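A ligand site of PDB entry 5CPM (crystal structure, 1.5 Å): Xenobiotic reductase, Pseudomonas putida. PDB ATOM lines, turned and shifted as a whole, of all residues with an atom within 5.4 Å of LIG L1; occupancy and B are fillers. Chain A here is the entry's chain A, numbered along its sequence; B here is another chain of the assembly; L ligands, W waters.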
ATOM      1  N   PRO A  22     -13.520  31.436  30.231  1.00  0.00           N
ATOM      2  CA  PRO A  22     -14.754  30.776  29.803  1.00  0.00           C
ATOM      3  C   PRO A  22     -14.460  29.365  29.334  1.00  0.00           C
ATOM      4  O   PRO A  22     -13.296  29.043  29.064  1.00  0.00           O
ATOM      5  CB  PRO A  22     -15.247  31.662  28.658  1.00  0.00           C
ATOM      6  CG  PRO A  22     -13.952  32.146  28.034  1.00  0.00           C
ATOM      7  CD  PRO A  22     -12.987  32.331  29.184  1.00  0.00           C
ATOM      8  N   PRO A  23     -15.491  28.517  29.236  1.00  0.00           N
ATOM      9  CA  PRO A  23     -15.270  27.157  28.751  1.00  0.00           C
ATOM     10  C   PRO A  23     -14.664  27.151  27.350  1.00  0.00           C
ATOM     11  O   PRO A  23     -15.150  27.879  26.476  1.00  0.00           O
ATOM     12  CB  PRO A  23     -16.685  26.558  28.766  1.00  0.00           C
ATOM     13  CG  PRO A  23     -17.617  27.774  28.668  1.00  0.00           C
ATOM     14  CD  PRO A  23     -16.911  28.818  29.481  1.00  0.00           C
ATOM     15  N   MET A  24     -13.604  26.380  27.151  1.00  0.00           N
ATOM     16  CA  MET A  24     -13.006  26.211  25.829  1.00  0.00           C
ATOM     17  C   MET A  24     -12.648  24.753  25.552  1.00  0.00           C
ATOM     18  O   MET A  24     -11.692  24.211  26.108  1.00  0.00           O
ATOM     19  CB  MET A  24     -11.742  27.082  25.670  1.00  0.00           C
ATOM     20  CG  MET A  24     -12.041  28.567  25.528  1.00  0.00           C
ATOM     21  SD  MET A  24     -10.534  29.567  25.430  1.00  0.00           S
ATOM     22  CE  MET A  24      -9.879  29.398  27.086  1.00  0.00           C
ATOM     23  N   CYS A  25     -13.440  24.131  24.685  1.00  0.00           N
ATOM     24  CA  CYS A  25     -13.197  22.765  24.220  1.00  0.00           C
ATOM     25  C   CYS A  25     -11.757  22.570  23.773  1.00  0.00           C
ATOM     26  O   CYS A  25     -11.198  23.406  23.053  1.00  0.00           O
ATOM     27  CB  CYS A  25     -14.132  22.440  23.065  1.00  0.00           C
ATOM     28  SG  CYS A  25     -15.833  22.130  23.595  1.00  0.00           S
ATOM     29  N   GLN A  26     -11.173  21.455  24.211  1.00  0.00           N
ATOM     30  CA  GLN A  26      -9.791  21.117  23.891  1.00  0.00           C
ATOM     31  C   GLN A  26      -9.717  19.993  22.857  1.00  0.00           C
ATOM     32  O   GLN A  26      -8.691  19.815  22.184  1.00  0.00           O
ATOM     33  CB  GLN A  26      -9.046  20.730  25.165  1.00  0.00           C
ATOM     34  CG  GLN A  26      -8.889  21.894  26.156  1.00  0.00           C
ATOM     35  CD  GLN A  26      -8.109  23.053  25.554  1.00  0.00           C
ATOM     36  OE1 GLN A  26      -6.898  22.976  25.384  1.00  0.00           O
ATOM     37  NE2 GLN A  26      -8.796  24.149  25.233  1.00  0.00           N
ATOM     38  N   TYR A  27     -10.812  19.234  22.737  1.00  0.00           N
ATOM     39  CA  TYR A  27     -10.928  18.137  21.787  1.00  0.00           C
ATOM     40  C   TYR A  27      -9.822  17.093  21.965  1.00  0.00           C
ATOM     41  O   TYR A  27      -9.399  16.469  20.996  1.00  0.00           O
ATOM     42  CB  TYR A  27     -10.920  18.660  20.342  1.00  0.00           C
ATOM     43  CG  TYR A  27     -11.887  19.804  20.095  1.00  0.00           C
ATOM     44  CD1 TYR A  27     -11.487  21.119  20.247  1.00  0.00           C
ATOM     45  CD2 TYR A  27     -13.205  19.561  19.725  1.00  0.00           C
ATOM     46  CE1 TYR A  27     -12.354  22.183  20.032  1.00  0.00           C
ATOM     47  CE2 TYR A  27     -14.095  20.622  19.494  1.00  0.00           C
ATOM     48  CZ  TYR A  27     -13.664  21.929  19.665  1.00  0.00           C
ATOM     49  OH  TYR A  27     -14.513  22.994  19.435  1.00  0.00           O
ATOM     50  N   GLU A  56     -14.271  23.442  30.011  1.00  0.00           N
ATOM     51  CA  GLU A  56     -14.903  23.261  28.701  1.00  0.00           C
ATOM     52  C   GLU A  56     -16.214  22.492  28.697  1.00  0.00           C
ATOM     53  O   GLU A  56     -16.490  21.705  29.613  1.00  0.00           O
ATOM     54  CB  GLU A  56     -13.930  22.535  27.767  1.00  0.00           C
ATOM     55  CG  GLU A  56     -13.663  21.080  28.190  1.00  0.00           C
ATOM     56  CD  GLU A  56     -12.412  20.527  27.533  1.00  0.00           C
ATOM     57  OE1 GLU A  56     -12.538  19.969  26.422  1.00  0.00           O
ATOM     58  OE2 GLU A  56     -11.319  20.665  28.125  1.00  0.00           O
ATOM     59  N   ALA A  57     -17.011  22.713  27.654  1.00  0.00           N
ATOM     60  CA  ALA A  57     -18.259  21.977  27.425  1.00  0.00           C
ATOM     61  C   ALA A  57     -18.059  20.481  27.626  1.00  0.00           C
ATOM     62  O   ALA A  57     -17.314  19.834  26.884  1.00  0.00           O
ATOM     63  CB  ALA A  57     -18.795  22.256  26.040  1.00  0.00           C
ATOM     64  N   GLN A  99     -18.768  23.664  32.567  1.00  0.00           N
ATOM     65  CA  GLN A  99     -19.924  23.803  31.700  1.00  0.00           C
ATOM     66  C   GLN A  99     -20.414  22.418  31.277  1.00  0.00           C
ATOM     67  O   GLN A  99     -19.671  21.650  30.661  1.00  0.00           O
ATOM     68  CB  GLN A  99     -19.579  24.650  30.470  1.00  0.00           C
ATOM     69  CG  GLN A  99     -20.792  24.951  29.594  1.00  0.00           C
ATOM     70  CD  GLN A  99     -20.390  25.549  28.277  1.00  0.00           C
ATOM     71  OE1 GLN A  99     -19.662  24.936  27.502  1.00  0.00           O
ATOM     72  NE2 GLN A  99     -20.846  26.773  28.009  1.00  0.00           N
ATOM     73  N   GLU A 176     -22.220  25.741  34.975  1.00  0.00           N
ATOM     74  CA  GLU A 176     -22.819  26.498  33.871  1.00  0.00           C
ATOM     75  C   GLU A 176     -23.558  25.565  32.922  1.00  0.00           C
ATOM     76  O   GLU A 176     -22.968  24.652  32.342  1.00  0.00           O
ATOM     77  CB  GLU A 176     -21.740  27.283  33.116  1.00  0.00           C
ATOM     78  CG  GLU A 176     -22.268  28.180  32.007  1.00  0.00           C
ATOM     79  CD  GLU A 176     -21.155  28.882  31.256  1.00  0.00           C
ATOM     80  OE1 GLU A 176     -20.475  29.731  31.867  1.00  0.00           O
ATOM     81  OE2 GLU A 176     -20.941  28.585  30.066  1.00  0.00           O
ATOM     82  N   HIS A 178     -25.060  24.737  29.452  1.00  0.00           N
ATOM     83  CA  HIS A 178     -24.767  25.238  28.098  1.00  0.00           C
ATOM     84  C   HIS A 178     -26.027  25.323  27.242  1.00  0.00           C
ATOM     85  O   HIS A 178     -26.377  24.398  26.514  1.00  0.00           O
ATOM     86  CB  HIS A 178     -23.739  24.362  27.400  1.00  0.00           C
ATOM     87  CG  HIS A 178     -23.091  25.052  26.235  1.00  0.00           C
ATOM     88  ND1 HIS A 178     -23.566  26.233  25.714  1.00  0.00           N
ATOM     89  CD2 HIS A 178     -21.991  24.736  25.504  1.00  0.00           C
ATOM     90  CE1 HIS A 178     -22.793  26.619  24.713  1.00  0.00           C
ATOM     91  NE2 HIS A 178     -21.828  25.720  24.565  1.00  0.00           N
ATOM     92  N   HIS A 181     -25.096  28.775  21.644  1.00  0.00           N
ATOM     93  CA  HIS A 181     -24.233  28.387  20.530  1.00  0.00           C
ATOM     94  C   HIS A 181     -24.834  27.303  19.645  1.00  0.00           C
ATOM     95  O   HIS A 181     -24.112  26.567  18.966  1.00  0.00           O
ATOM     96  CB  HIS A 181     -22.845  27.953  21.049  1.00  0.00           C
ATOM     97  CG  HIS A 181     -22.136  29.026  21.828  1.00  0.00           C
ATOM     98  ND1 HIS A 181     -20.947  28.810  22.510  1.00  0.00           N
ATOM     99  CD2 HIS A 181     -22.453  30.336  22.035  1.00  0.00           C
ATOM    100  CE1 HIS A 181     -20.570  29.934  23.097  1.00  0.00           C
ATOM    101  NE2 HIS A 181     -21.463  30.869  22.830  1.00  0.00           N
ATOM    102  N   ARG A 231     -25.160  29.608  30.138  1.00  0.00           N
ATOM    103  CA  ARG A 231     -24.791  30.396  28.961  1.00  0.00           C
ATOM    104  C   ARG A 231     -25.938  30.324  27.968  1.00  0.00           C
ATOM    105  O   ARG A 231     -26.534  29.259  27.778  1.00  0.00           O
ATOM    106  CB  ARG A 231     -23.487  29.880  28.333  1.00  0.00           C
ATOM    107  CG  ARG A 231     -22.853  30.892  27.392  1.00  0.00           C
ATOM    108  CD  ARG A 231     -21.390  30.554  27.055  1.00  0.00           C
ATOM    109  NE  ARG A 231     -20.633  31.772  26.753  1.00  0.00           N
ATOM    110  CZ  ARG A 231     -19.364  31.794  26.354  1.00  0.00           C
ATOM    111  NH1 ARG A 231     -18.708  30.658  26.147  1.00  0.00           N
ATOM    112  NH2 ARG A 231     -18.766  32.953  26.131  1.00  0.00           N
ATOM    113  N   ALA A 301     -18.091  37.658  26.446  1.00  0.00           N
ATOM    114  CA  ALA A 301     -16.793  37.408  25.866  1.00  0.00           C
ATOM    115  C   ALA A 301     -16.688  37.974  24.460  1.00  0.00           C
ATOM    116  O   ALA A 301     -17.618  38.625  23.986  1.00  0.00           O
ATOM    117  CB  ALA A 301     -16.515  35.908  25.865  1.00  0.00           C
ATOM    118  N   TRP A 302     -15.525  37.734  23.849  1.00  0.00           N
ATOM    119  CA  TRP A 302     -15.122  38.096  22.473  1.00  0.00           C
ATOM    120  C   TRP A 302     -14.363  39.426  22.400  1.00  0.00           C
ATOM    121  O   TRP A 302     -14.942  40.508  22.239  1.00  0.00           O
ATOM    122  CB  TRP A 302     -16.311  38.102  21.491  1.00  0.00           C
ATOM    123  CG  TRP A 302     -16.631  36.726  21.006  1.00  0.00           C
ATOM    124  CD1 TRP A 302     -16.008  36.048  19.994  1.00  0.00           C
ATOM    125  CD2 TRP A 302     -17.629  35.833  21.524  1.00  0.00           C
ATOM    126  NE1 TRP A 302     -16.558  34.795  19.849  1.00  0.00           N
ATOM    127  CE2 TRP A 302     -17.558  34.636  20.773  1.00  0.00           C
ATOM    128  CE3 TRP A 302     -18.580  35.930  22.544  1.00  0.00           C
ATOM    129  CZ2 TRP A 302     -18.395  33.551  21.017  1.00  0.00           C
ATOM    130  CZ3 TRP A 302     -19.416  34.853  22.783  1.00  0.00           C
ATOM    131  CH2 TRP A 302     -19.320  33.679  22.018  1.00  0.00           C
ATOM    132  N   GLY A 303     -13.035  39.313  22.495  1.00  0.00           N
ATOM    133  CA  GLY A 303     -12.164  40.456  22.342  1.00  0.00           C
ATOM    134  C   GLY A 303     -11.709  41.154  23.601  1.00  0.00           C
ATOM    135  O   GLY A 303     -11.086  42.208  23.526  1.00  0.00           O
ATOM    136  N   PHE A 304     -12.007  40.594  24.771  1.00  0.00           N
ATOM    137  CA  PHE A 304     -11.662  41.278  26.004  1.00  0.00           C
ATOM    138  C   PHE A 304     -10.227  40.988  26.466  1.00  0.00           C
ATOM    139  O   PHE A 304      -9.846  41.363  27.564  1.00  0.00           O
ATOM    140  CB  PHE A 304     -12.651  40.933  27.112  1.00  0.00           C
ATOM    141  CG  PHE A 304     -14.008  41.554  26.928  1.00  0.00           C
ATOM    142  CD1 PHE A 304     -14.207  42.913  27.167  1.00  0.00           C
ATOM    143  CD2 PHE A 304     -15.081  40.787  26.498  1.00  0.00           C
ATOM    144  CE1 PHE A 304     -15.462  43.477  26.996  1.00  0.00           C
ATOM    145  CE2 PHE A 304     -16.328  41.346  26.316  1.00  0.00           C
ATOM    146  CZ  PHE A 304     -16.517  42.697  26.568  1.00  0.00           C
ATOM    147  N   GLY A 305      -9.442  40.357  25.599  1.00  0.00           N
ATOM    148  CA  GLY A 305      -8.023  40.135  25.883  1.00  0.00           C
ATOM    149  C   GLY A 305      -7.186  41.396  25.910  1.00  0.00           C
ATOM    150  O   GLY A 305      -6.017  41.379  26.307  1.00  0.00           O
ATOM    151  N   SER A 323     -15.010  37.552  30.653  1.00  0.00           N
ATOM    152  CA  SER A 323     -14.492  36.274  30.170  1.00  0.00           C
ATOM    153  C   SER A 323     -13.435  36.490  29.100  1.00  0.00           C
ATOM    154  O   SER A 323     -13.682  37.187  28.122  1.00  0.00           O
ATOM    155  CB  SER A 323     -15.622  35.407  29.617  1.00  0.00           C
ATOM    156  OG  SER A 323     -16.485  35.008  30.676  1.00  0.00           O
ATOM    157  N   VAL A 324     -12.259  35.884  29.294  1.00  0.00           N
ATOM    158  CA  VAL A 324     -11.097  36.048  28.421  1.00  0.00           C
ATOM    159  C   VAL A 324     -10.635  34.659  28.017  1.00  0.00           C
ATOM    160  O   VAL A 324     -10.052  33.934  28.836  1.00  0.00           O
ATOM    161  CB  VAL A 324      -9.997  36.840  29.120  1.00  0.00           C
ATOM    162  CG1 VAL A 324      -8.756  37.001  28.221  1.00  0.00           C
ATOM    163  CG2 VAL A 324     -10.529  38.216  29.567  1.00  0.00           C
ATOM    164  N   GLY A 325     -10.889  34.295  26.767  1.00  0.00           N
ATOM    165  CA  GLY A 325     -10.641  32.955  26.290  1.00  0.00           C
ATOM    166  C   GLY A 325      -9.342  32.764  25.520  1.00  0.00           C
ATOM    167  O   GLY A 325      -8.352  32.284  26.077  1.00  0.00           O
ATOM    168  N   ARG A 326      -9.355  33.145  24.247  1.00  0.00           N
ATOM    169  CA  ARG A 326      -8.209  32.880  23.375  1.00  0.00           C
ATOM    170  C   ARG A 326      -6.899  33.504  23.900  1.00  0.00           C
ATOM    171  O   ARG A 326      -5.835  32.914  23.738  1.00  0.00           O
ATOM    172  CB  ARG A 326      -8.494  33.374  21.949  1.00  0.00           C
ATOM    173  CG  ARG A 326      -9.343  32.375  21.159  1.00  0.00           C
ATOM    174  CD  ARG A 326      -9.922  32.958  19.869  1.00  0.00           C
ATOM    175  NE  ARG A 326     -10.860  34.036  20.159  1.00  0.00           N
ATOM    176  CZ  ARG A 326     -11.465  34.772  19.230  1.00  0.00           C
ATOM    177  NH1 ARG A 326     -11.215  34.549  17.948  1.00  0.00           N
ATOM    178  NH2 ARG A 326     -12.295  35.748  19.582  1.00  0.00           N
ATOM    179  N   ALA A 327      -6.980  34.662  24.559  1.00  0.00           N
ATOM    180  CA  ALA A 327      -5.772  35.270  25.134  1.00  0.00           C
ATOM    181  C   ALA A 327      -5.102  34.357  26.165  1.00  0.00           C
ATOM    182  O   ALA A 327      -3.900  34.443  26.382  1.00  0.00           O
ATOM    183  CB  ALA A 327      -6.091  36.628  25.751  1.00  0.00           C
ATOM    184  N   LEU A 329      -5.219  30.991  25.893  1.00  0.00           N
ATOM    185  CA  LEU A 329      -4.581  29.939  25.118  1.00  0.00           C
ATOM    186  C   LEU A 329      -3.215  30.425  24.653  1.00  0.00           C
ATOM    187  O   LEU A 329      -2.235  29.680  24.682  1.00  0.00           O
ATOM    188  CB  LEU A 329      -5.434  29.552  23.905  1.00  0.00           C
ATOM    189  CG  LEU A 329      -6.880  29.162  24.204  1.00  0.00           C
ATOM    190  CD1 LEU A 329      -7.551  28.810  22.894  1.00  0.00           C
ATOM    191  CD2 LEU A 329      -6.974  28.002  25.200  1.00  0.00           C
ATOM    192  N   PRO B 354      -4.594  22.255  19.855  1.00  0.00           N
ATOM    193  CA  PRO B 354      -5.766  22.835  20.528  1.00  0.00           C
ATOM    194  C   PRO B 354      -5.649  24.329  20.822  1.00  0.00           C
ATOM    195  O   PRO B 354      -6.660  24.991  21.119  1.00  0.00           O
ATOM    196  CB  PRO B 354      -5.825  22.059  21.855  1.00  0.00           C
ATOM    197  CG  PRO B 354      -5.133  20.758  21.565  1.00  0.00           C
ATOM    198  CD  PRO B 354      -4.014  21.139  20.613  1.00  0.00           C
ATOM    199  N   TRP B 358      -6.751  27.930  16.836  1.00  0.00           N
ATOM    200  CA  TRP B 358      -7.599  29.073  17.158  1.00  0.00           C
ATOM    201  C   TRP B 358      -6.836  30.394  17.142  1.00  0.00           C
ATOM    202  O   TRP B 358      -7.432  31.469  17.108  1.00  0.00           O
ATOM    203  CB  TRP B 358      -8.253  28.844  18.510  1.00  0.00           C
ATOM    204  CG  TRP B 358      -9.081  27.596  18.542  1.00  0.00           C
ATOM    205  CD1 TRP B 358      -8.697  26.361  19.006  1.00  0.00           C
ATOM    206  CD2 TRP B 358     -10.430  27.448  18.075  1.00  0.00           C
ATOM    207  NE1 TRP B 358      -9.725  25.459  18.863  1.00  0.00           N
ATOM    208  CE2 TRP B 358     -10.803  26.103  18.292  1.00  0.00           C
ATOM    209  CE3 TRP B 358     -11.354  28.319  17.500  1.00  0.00           C
ATOM    210  CZ2 TRP B 358     -12.068  25.615  17.966  1.00  0.00           C
ATOM    211  CZ3 TRP B 358     -12.610  27.834  17.159  1.00  0.00           C
ATOM    212  CH2 TRP B 358     -12.958  26.496  17.401  1.00  0.00           C
HETATM  213  C1  LIG L   1     -14.710  28.248  22.550  1.00  0.00           C
HETATM  214  N1  LIG L   1     -15.907  28.770  23.207  1.00  0.00           N
HETATM  215  C2  LIG L   1     -16.785  27.905  23.986  1.00  0.00           C
HETATM  216  N2  LIG L   1     -17.967  28.354  24.384  1.00  0.00           N
HETATM  217  C3  LIG L   1     -18.701  27.586  25.236  1.00  0.00           C
HETATM  218  O1  LIG L   1     -19.728  28.020  25.662  1.00  0.00           O
HETATM  219  N3  LIG L   1     -18.241  26.333  25.590  1.00  0.00           N
HETATM  220  C4  LIG L   1     -17.096  25.856  25.113  1.00  0.00           C
HETATM  221  O2  LIG L   1     -16.697  24.763  25.427  1.00  0.00           O
HETATM  222  C5  LIG L   1     -16.485  26.574  24.099  1.00  0.00           C
HETATM  223  N4  LIG L   1     -15.306  26.029  23.432  1.00  0.00           N
HETATM  224  C6  LIG L   1     -14.424  26.901  22.672  1.00  0.00           C
HETATM  225  C7  LIG L   1     -13.144  26.440  22.335  1.00  0.00           C
HETATM  226  C8  LIG L   1     -12.194  27.332  21.849  1.00  0.00           C
HETATM  227  C9  LIG L   1     -10.785  26.784  21.641  1.00  0.00           C
HETATM  228  C10 LIG L   1     -12.576  28.654  21.581  1.00  0.00           C
HETATM  229  C11 LIG L   1     -11.531  29.628  21.042  1.00  0.00           C
HETATM  230  C12 LIG L   1     -13.867  29.077  21.804  1.00  0.00           C
HETATM  231  C13 LIG L   1     -16.201  30.194  23.132  1.00  0.00           C
HETATM  232  C14 LIG L   1     -15.372  30.906  24.219  1.00  0.00           C
HETATM  233  O3  LIG L   1     -15.800  30.522  25.510  1.00  0.00           O
HETATM  234  C15 LIG L   1     -15.410  32.434  24.103  1.00  0.00           C
HETATM  235  O4  LIG L   1     -16.743  32.920  24.199  1.00  0.00           O
HETATM  236  C16 LIG L   1     -14.793  32.891  22.775  1.00  0.00           C
HETATM  237  O5  LIG L   1     -13.496  32.355  22.553  1.00  0.00           O
HETATM  238  C17 LIG L   1     -14.711  34.420  22.710  1.00  0.00           C
HETATM  239  O6  LIG L   1     -13.894  34.936  23.724  1.00  0.00           O
HETATM  240  P1  LIG L   1     -12.344  35.391  23.388  1.00  0.00           P
HETATM  241  O7  LIG L   1     -11.645  34.165  22.845  1.00  0.00           O
HETATM  242  O8  LIG L   1     -12.376  36.477  22.350  1.00  0.00           O
HETATM  243  O9  LIG L   1     -11.750  35.871  24.684  1.00  0.00           O
HETATM  244  P1  LG2 L   2     -15.654  31.931  13.528  1.00  0.00           P
HETATM  245  O1  LG2 L   2     -15.143  33.041  14.388  1.00  0.00           O
HETATM  246  O2  LG2 L   2     -14.761  30.800  13.126  1.00  0.00           O
HETATM  247  O3  LG2 L   2     -16.399  32.577  12.192  1.00  0.00           O
HETATM  248  C1  LG2 L   2     -16.244  33.955  12.338  1.00  0.00           C
HETATM  249  C2  LG2 L   2     -14.871  34.343  11.856  1.00  0.00           C
HETATM  250  O4  LG2 L   2     -14.897  34.595  10.462  1.00  0.00           O
HETATM  251  C3  LG2 L   2     -14.473  35.621  12.574  1.00  0.00           C
HETATM  252  C4  LG2 L   2     -13.383  36.150  11.623  1.00  0.00           C
HETATM  253  O5  LG2 L   2     -12.171  35.666  11.881  1.00  0.00           O
HETATM  254  C5  LG2 L   2     -13.903  35.599  10.219  1.00  0.00           C
HETATM  255  O6  LG2 L   2     -16.809  31.353  14.545  1.00  0.00           O
HETATM  256  P2  LG2 L   2     -17.527  30.047  13.962  1.00  0.00           P
HETATM  257  O7  LG2 L   2     -16.547  28.984  13.646  1.00  0.00           O
HETATM  258  O8  LG2 L   2     -18.772  30.315  13.149  1.00  0.00           O
HETATM  259  O9  LG2 L   2     -18.240  29.361  15.435  1.00  0.00           O
HETATM  260  C6  LG2 L   2     -18.712  30.467  16.121  1.00  0.00           C
HETATM  261  C7  LG2 L   2     -18.162  30.495  17.554  1.00  0.00           C
HETATM  262  O10 LG2 L   2     -18.391  29.278  18.217  1.00  0.00           O
HETATM  263  C8  LG2 L   2     -16.613  30.589  17.551  1.00  0.00           C
HETATM  264  O11 LG2 L   2     -16.242  31.919  17.351  1.00  0.00           O
HETATM  265  C9  LG2 L   2     -16.281  30.121  18.979  1.00  0.00           C
HETATM  266  O12 LG2 L   2     -16.141  31.174  19.864  1.00  0.00           O
HETATM  267  C10 LG2 L   2     -17.590  29.330  19.378  1.00  0.00           C
HETATM  268  N1  LG2 L   2     -17.276  27.958  19.780  1.00  0.00           N
HETATM  269  C11 LG2 L   2     -18.011  27.411  20.806  1.00  0.00           C
HETATM  270  C12 LG2 L   2     -17.933  26.094  21.114  1.00  0.00           C
HETATM  271  C13 LG2 L   2     -18.783  25.640  22.204  1.00  0.00           C
HETATM  272  O13 LG2 L   2     -19.696  26.315  22.695  1.00  0.00           O
HETATM  273  N2  LG2 L   2     -18.533  24.377  22.728  1.00  0.00           N
HETATM  274  C14 LG2 L   2     -17.018  25.151  20.368  1.00  0.00           C
HETATM  275  C15 LG2 L   2     -16.202  25.872  19.342  1.00  0.00           C
HETATM  276  C16 LG2 L   2     -16.327  27.179  19.092  1.00  0.00           C
HETATM  277  O   HOH W   1      -9.115  36.572  24.655  1.00  0.00           O
HETATM  278  O   HOH W   2     -10.178  37.565  21.223  1.00  0.00           O
HETATM  279  O   HOH W   3     -13.136  37.996  25.535  1.00  0.00           O
HETATM  280  O   HOH W   4     -13.814  32.327  19.608  1.00  0.00           O
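An oxygen (O9) of LIG L1 sits at hydrogen-bond distance from the backbone NH (N) of Gly 325, 2.8 Å away.
N3 of LIG L1 is in hydrogen-bond range of OE1 of Gln 99 (2.8 Å).
An oxygen (O4) of LIG L1 is in hydrogen-bond range of the guanidinium group (NH2) of Arg 231.
The backbone NH (N) of Arg 326 lies within hydrogen-bond range of an oxygen (O7) of LIG L1 (2.9 Å).
NE of Arg 326 lies within salt-bridge range of O7 of LIG L1, at 2.8 Å.
O3 of LIG L1 is in hydrogen-bond range of O of Pro 23 (2.9 Å).
N of Gly 303 sits at hydrogen-bond distance from O8 of LIG L1, 2.9 Å away.
N of Cys 25 sits close to O2 of LIG L1 (3.4 Å).
O2 of LIG L1 is in hydrogen-bond range of SG of Cys 25, 3.3 Å away.
The backbone NH (N) of Ala 57 sits at hydrogen-bond distance from an oxygen (O2) of LIG L1, 3.0 Å away.
The backbone NH of Trp 302 lies within hydrogen-bond range of an oxygen (O6) of LIG L1.
An oxygen (O1) of LIG L1 is in hydrogen-bond range of a ring nitrogen (NE2) of His 178, 3.3 Å away.
A ring nitrogen (ND1) of His 181 lies close to an oxygen (O1) of LIG L1 (3.5 Å).
The side-chain sulfur (SG) of Cys 25 lies within hydrogen-bond range of a nitrogen (N2) of LG2 L2 (3.6 Å).
O13 of LG2 L2 is in hydrogen-bond range of NE2 of His 178.
O13 of LG2 L2 lies within hydrogen-bond range of ND1 of His 181, at 2.8 Å.
A nitrogen (N2) of LIG L1 lies close to an oxygen (O13) of LG2 L2 (3.2 Å).
The side-chain amide oxygen of Gln 99 sits close to the backbone NH of Ala 57 (3.5 Å).
The side-chain amide nitrogen of Gln 99 sits at hydrogen-bond distance from the side-chain carboxylate of Glu 176 (2.7 Å).
The backbone carbonyl oxygen of Met 24 lies within hydrogen-bond range of the side-chain amide nitrogen of Gln 26, 3.0 Å away.
Pro 22 touches LIG L1.
Met 24 touches LIG L1 (CA to N4, 3.3 Å).
Ala 301 touches LIG L1 (CB to O4, 3.4 Å).
Val 324 touches LIG L1.
NE1 of Trp 358 of chain B touches C9 of LIG L1, at 3.3 Å.
Within 4 Å of LIG L1: Pro 22, Pro 23, Met 24, Cys 25, Ala 57, Gln 99, His 178, His 181, Arg 231, Ala 301, Trp 302, Gly 303, Val 324, Gly 325, Arg 326 and Trp 358 of chain B.
The nearest printed residue that does not touch LIG L1 is Glu 56 (4.01 Å).
Water W2 bridges an oxygen (O8) of LIG L1 (2.7 Å) and the guanidinium group (NH2) of Arg 326 (3.2 Å).
Water W1 lies within hydrogen-bond range of O9 of LIG L1, N of Ala 327 and N of Arg 326.
Water W4 lies within hydrogen-bond range of O12 of LG2 L2 (2.6 Å), O5 of LIG L1 (3.0 Å) and NE of Arg 326 (3.5 Å).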
